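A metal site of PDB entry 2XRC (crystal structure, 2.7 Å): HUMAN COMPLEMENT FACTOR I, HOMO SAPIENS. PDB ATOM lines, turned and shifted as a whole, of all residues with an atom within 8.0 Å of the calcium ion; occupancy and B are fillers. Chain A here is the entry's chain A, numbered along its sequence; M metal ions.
The calcium ion is bound by OD2 of Asp 265 (2.1 Å), O of Tyr 258 (2.1 Å), OD1 of Asn 261 (2.3 Å), O of Glu 263 (2.3 Å), OD2 of Asp 271 (2.5 Å) and OE1 of Glu 272 (2.7 Å).
Of the 19 residues printed, 6 come within 4 Å of the calcium ion. Along chain A the residues within 4 Å of the calcium ion span positions 258 to 272.
The side-chain sulfur (SG) of Cys 260 is disulfide-bonded to the side-chain sulfur (SG) of Cys 275 (2.0 Å). The side-chain carboxylate (OE1) of Glu 272 sits close to the backbone NH (N) of Cys 260 (3.1 Å). The backbone NH of Gly 262 lies within hydrogen-bond range of the side-chain carboxylate of Glu 272 (3.0 Å). The backbone carbonyl oxygen (O) of Asp 271 is in hydrogen-bond range of the backbone NH (N) of Cys 260 (3.1 Å).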
ATOM      1  N   ILE A 254     -27.880  -3.126 -24.986  1.00  0.00           N
ATOM      2  CA  ILE A 254     -28.178  -2.173 -26.062  1.00  0.00           C
ATOM      3  C   ILE A 254     -27.859  -2.784 -27.430  1.00  0.00           C
ATOM      4  O   ILE A 254     -27.013  -3.687 -27.522  1.00  0.00           O
ATOM      5  CB  ILE A 254     -27.410  -0.833 -25.878  1.00  0.00           C
ATOM      6  CG1 ILE A 254     -25.897  -1.027 -25.977  1.00  0.00           C
ATOM      7  CG2 ILE A 254     -27.767  -0.193 -24.546  1.00  0.00           C
ATOM      8  CD1 ILE A 254     -25.091   0.239 -25.693  1.00  0.00           C
ATOM      9  N   PRO A 255     -28.542  -2.322 -28.490  1.00  0.00           N
ATOM     10  CA  PRO A 255     -28.233  -2.844 -29.831  1.00  0.00           C
ATOM     11  C   PRO A 255     -26.773  -2.605 -30.227  1.00  0.00           C
ATOM     12  O   PRO A 255     -26.264  -1.512 -30.032  1.00  0.00           O
ATOM     13  CB  PRO A 255     -29.168  -2.032 -30.745  1.00  0.00           C
ATOM     14  CG  PRO A 255     -30.278  -1.600 -29.868  1.00  0.00           C
ATOM     15  CD  PRO A 255     -29.683  -1.386 -28.513  1.00  0.00           C
ATOM     16  N   SER A 256     -26.119  -3.625 -30.777  1.00  0.00           N
ATOM     17  CA  SER A 256     -24.708  -3.519 -31.179  1.00  0.00           C
ATOM     18  C   SER A 256     -24.383  -2.216 -31.912  1.00  0.00           C
ATOM     19  O   SER A 256     -23.349  -1.614 -31.661  1.00  0.00           O
ATOM     20  CB  SER A 256     -24.316  -4.693 -32.076  1.00  0.00           C
ATOM     21  OG  SER A 256     -24.827  -5.910 -31.597  1.00  0.00           O
ATOM     22  N   GLN A 257     -25.269  -1.795 -32.810  1.00  0.00           N
ATOM     23  CA  GLN A 257     -25.048  -0.549 -33.579  1.00  0.00           C
ATOM     24  C   GLN A 257     -25.163   0.717 -32.719  1.00  0.00           C
ATOM     25  O   GLN A 257     -24.850   1.819 -33.173  1.00  0.00           O
ATOM     26  CB  GLN A 257     -25.933  -0.436 -34.833  1.00  0.00           C
ATOM     27  CG  GLN A 257     -27.311  -1.106 -34.786  1.00  0.00           C
ATOM     28  CD  GLN A 257     -27.260  -2.547 -35.254  1.00  0.00           C
ATOM     29  OE1 GLN A 257     -26.411  -3.336 -34.817  1.00  0.00           O
ATOM     30  NE2 GLN A 257     -28.171  -2.920 -36.149  1.00  0.00           N
ATOM     31  N   TYR A 258     -25.607   0.557 -31.479  1.00  0.00           N
ATOM     32  CA  TYR A 258     -25.523   1.625 -30.474  1.00  0.00           C
ATOM     33  C   TYR A 258     -24.086   1.812 -29.964  1.00  0.00           C
ATOM     34  O   TYR A 258     -23.828   2.722 -29.175  1.00  0.00           O
ATOM     35  CB  TYR A 258     -26.466   1.340 -29.290  1.00  0.00           C
ATOM     36  CG  TYR A 258     -27.903   1.763 -29.523  1.00  0.00           C
ATOM     37  CD1 TYR A 258     -28.523   1.607 -30.773  1.00  0.00           C
ATOM     38  CD2 TYR A 258     -28.669   2.301 -28.483  1.00  0.00           C
ATOM     39  CE1 TYR A 258     -29.835   2.004 -30.970  1.00  0.00           C
ATOM     40  CE2 TYR A 258     -29.986   2.690 -28.677  1.00  0.00           C
ATOM     41  CZ  TYR A 258     -30.565   2.539 -29.921  1.00  0.00           C
ATOM     42  OH  TYR A 258     -31.870   2.924 -30.107  1.00  0.00           O
ATOM     43  N   GLN A 259     -23.166   0.951 -30.410  1.00  0.00           N
ATOM     44  CA  GLN A 259     -21.728   1.134 -30.140  1.00  0.00           C
ATOM     45  C   GLN A 259     -21.110   2.158 -31.085  1.00  0.00           C
ATOM     46  O   GLN A 259     -21.236   2.048 -32.301  1.00  0.00           O
ATOM     47  CB  GLN A 259     -20.964  -0.192 -30.281  1.00  0.00           C
ATOM     48  CG  GLN A 259     -21.320  -1.238 -29.233  1.00  0.00           C
ATOM     49  CD  GLN A 259     -20.342  -2.400 -29.207  1.00  0.00           C
ATOM     50  OE1 GLN A 259     -19.613  -2.583 -28.227  1.00  0.00           O
ATOM     51  NE2 GLN A 259     -20.314  -3.161 -30.290  1.00  0.00           N
ATOM     52  N   CYS A 260     -20.431   3.146 -30.504  1.00  0.00           N
ATOM     53  CA  CYS A 260     -19.744   4.190 -31.261  1.00  0.00           C
ATOM     54  C   CYS A 260     -20.663   4.876 -32.283  1.00  0.00           C
ATOM     55  O   CYS A 260     -20.302   5.012 -33.454  1.00  0.00           O
ATOM     56  CB  CYS A 260     -18.511   3.621 -31.967  1.00  0.00           C
ATOM     57  SG  CYS A 260     -17.327   2.792 -30.870  1.00  0.00           S
ATOM     58  N   ASN A 261     -21.842   5.299 -31.826  1.00  0.00           N
ATOM     59  CA  ASN A 261     -22.809   5.997 -32.680  1.00  0.00           C
ATOM     60  C   ASN A 261     -23.019   7.458 -32.276  1.00  0.00           C
ATOM     61  O   ASN A 261     -23.953   8.116 -32.729  1.00  0.00           O
ATOM     62  CB  ASN A 261     -24.143   5.240 -32.728  1.00  0.00           C
ATOM     63  CG  ASN A 261     -24.931   5.334 -31.426  1.00  0.00           C
ATOM     64  OD1 ASN A 261     -24.389   5.610 -30.360  1.00  0.00           O
ATOM     65  ND2 ASN A 261     -26.239   5.078 -31.510  1.00  0.00           N
ATOM     66  N   GLY A 262     -22.135   7.975 -31.415  1.00  0.00           N
ATOM     67  CA  GLY A 262     -22.153   9.374 -31.004  1.00  0.00           C
ATOM     68  C   GLY A 262     -23.194   9.698 -29.954  1.00  0.00           C
ATOM     69  O   GLY A 262     -23.545  10.872 -29.749  1.00  0.00           O
ATOM     70  N   GLU A 263     -23.687   8.666 -29.273  1.00  0.00           N
ATOM     71  CA  GLU A 263     -24.629   8.839 -28.172  1.00  0.00           C
ATOM     72  C   GLU A 263     -24.255   7.902 -27.019  1.00  0.00           C
ATOM     73  O   GLU A 263     -24.205   6.680 -27.199  1.00  0.00           O
ATOM     74  CB  GLU A 263     -26.062   8.556 -28.617  1.00  0.00           C
ATOM     75  CG  GLU A 263     -27.122   9.089 -27.640  1.00  0.00           C
ATOM     76  CD  GLU A 263     -28.453   8.356 -27.739  1.00  0.00           C
ATOM     77  OE1 GLU A 263     -29.226   8.424 -26.765  1.00  0.00           O
ATOM     78  OE2 GLU A 263     -28.727   7.711 -28.779  1.00  0.00           O
ATOM     79  N   VAL A 264     -23.994   8.484 -25.862  1.00  0.00           N
ATOM     80  CA  VAL A 264     -23.760   7.705 -24.650  1.00  0.00           C
ATOM     81  C   VAL A 264     -25.087   7.071 -24.226  1.00  0.00           C
ATOM     82  O   VAL A 264     -25.942   7.743 -23.663  1.00  0.00           O
ATOM     83  CB  VAL A 264     -23.211   8.600 -23.507  1.00  0.00           C
ATOM     84  CG1 VAL A 264     -23.048   7.795 -22.218  1.00  0.00           C
ATOM     85  CG2 VAL A 264     -21.889   9.241 -23.920  1.00  0.00           C
ATOM     86  N   ASP A 265     -25.241   5.775 -24.519  1.00  0.00           N
ATOM     87  CA  ASP A 265     -26.448   5.035 -24.171  1.00  0.00           C
ATOM     88  C   ASP A 265     -26.391   4.456 -22.762  1.00  0.00           C
ATOM     89  O   ASP A 265     -27.240   4.767 -21.934  1.00  0.00           O
ATOM     90  CB  ASP A 265     -26.695   3.912 -25.167  1.00  0.00           C
ATOM     91  CG  ASP A 265     -27.064   4.423 -26.552  1.00  0.00           C
ATOM     92  OD1 ASP A 265     -28.142   5.027 -26.710  1.00  0.00           O
ATOM     93  OD2 ASP A 265     -26.266   4.204 -27.480  1.00  0.00           O
ATOM     94  N   CYS A 266     -25.393   3.609 -22.508  1.00  0.00           N
ATOM     95  CA  CYS A 266     -25.213   3.028 -21.178  1.00  0.00           C
ATOM     96  C   CYS A 266     -24.901   4.134 -20.170  1.00  0.00           C
ATOM     97  O   CYS A 266     -24.123   5.035 -20.469  1.00  0.00           O
ATOM     98  CB  CYS A 266     -24.067   2.005 -21.159  1.00  0.00           C
ATOM     99  SG  CYS A 266     -24.119   0.723 -22.433  1.00  0.00           S
ATOM    100  N   GLY A 269     -21.306   4.242 -19.722  1.00  0.00           N
ATOM    101  CA  GLY A 269     -20.730   5.044 -20.819  1.00  0.00           C
ATOM    102  C   GLY A 269     -19.742   4.323 -21.704  1.00  0.00           C
ATOM    103  O   GLY A 269     -18.981   4.959 -22.450  1.00  0.00           O
ATOM    104  N   GLU A 270     -19.752   2.996 -21.662  1.00  0.00           N
ATOM    105  CA  GLU A 270     -18.676   2.175 -22.220  1.00  0.00           C
ATOM    106  C   GLU A 270     -18.812   1.920 -23.705  1.00  0.00           C
ATOM    107  O   GLU A 270     -17.848   1.537 -24.363  1.00  0.00           O
ATOM    108  CB  GLU A 270     -18.609   0.841 -21.473  1.00  0.00           C
ATOM    109  CG  GLU A 270     -19.719  -0.125 -21.853  1.00  0.00           C
ATOM    110  CD  GLU A 270     -20.121  -1.043 -20.730  1.00  0.00           C
ATOM    111  OE1 GLU A 270     -20.600  -0.524 -19.695  1.00  0.00           O
ATOM    112  OE2 GLU A 270     -19.983  -2.272 -20.875  1.00  0.00           O
ATOM    113  N   ASP A 271     -20.022   2.108 -24.243  1.00  0.00           N
ATOM    114  CA  ASP A 271     -20.273   1.899 -25.674  1.00  0.00           C
ATOM    115  C   ASP A 271     -19.598   2.949 -26.547  1.00  0.00           C
ATOM    116  O   ASP A 271     -19.255   2.681 -27.697  1.00  0.00           O
ATOM    117  CB  ASP A 271     -21.784   1.835 -25.954  1.00  0.00           C
ATOM    118  CG  ASP A 271     -22.503   3.149 -25.642  1.00  0.00           C
ATOM    119  OD1 ASP A 271     -22.037   3.914 -24.767  1.00  0.00           O
ATOM    120  OD2 ASP A 271     -23.541   3.404 -26.292  1.00  0.00           O
ATOM    121  N   GLU A 272     -19.408   4.150 -26.005  1.00  0.00           N
ATOM    122  CA  GLU A 272     -18.781   5.262 -26.733  1.00  0.00           C
ATOM    123  C   GLU A 272     -17.293   5.450 -26.417  1.00  0.00           C
ATOM    124  O   GLU A 272     -16.645   6.299 -27.028  1.00  0.00           O
ATOM    125  CB  GLU A 272     -19.545   6.564 -26.478  1.00  0.00           C
ATOM    126  CG  GLU A 272     -20.977   6.562 -26.998  1.00  0.00           C
ATOM    127  CD  GLU A 272     -21.069   6.239 -28.474  1.00  0.00           C
ATOM    128  OE1 GLU A 272     -21.864   5.352 -28.848  1.00  0.00           O
ATOM    129  OE2 GLU A 272     -20.326   6.865 -29.267  1.00  0.00           O
ATOM    130  N   CYS A 275     -13.549   4.610 -29.568  1.00  0.00           N
ATOM    131  CA  CYS A 275     -14.135   4.811 -30.900  1.00  0.00           C
ATOM    132  C   CYS A 275     -13.309   5.824 -31.701  1.00  0.00           C
ATOM    133  O   CYS A 275     -13.480   7.043 -31.564  1.00  0.00           O
ATOM    134  CB  CYS A 275     -15.593   5.292 -30.766  1.00  0.00           C
ATOM    135  SG  CYS A 275     -16.624   4.281 -29.670  1.00  0.00           S
ATOM    136  N   ARG A 298     -31.076  13.082 -30.344  1.00  0.00           N
ATOM    137  CA  ARG A 298     -29.632  13.033 -30.101  1.00  0.00           C
ATOM    138  C   ARG A 298     -29.034  14.432 -30.129  1.00  0.00           C
ATOM    139  O   ARG A 298     -28.278  14.809 -29.242  1.00  0.00           O
ATOM    140  CB  ARG A 298     -28.937  12.121 -31.117  1.00  0.00           C
ATOM    141  CG  ARG A 298     -28.983  10.652 -30.745  1.00  0.00           C
ATOM    142  CD  ARG A 298     -28.466   9.758 -31.851  1.00  0.00           C
ATOM    143  NE  ARG A 298     -29.500   9.493 -32.844  1.00  0.00           N
ATOM    144  CZ  ARG A 298     -29.382   8.639 -33.864  1.00  0.00           C
ATOM    145  NH1 ARG A 298     -28.260   7.943 -34.041  1.00  0.00           N
ATOM    146  NH2 ARG A 298     -30.386   8.489 -34.719  1.00  0.00           N
HETATM  147 CA    CA M   1     -24.346   4.606 -28.293  1.00  0.00          CA
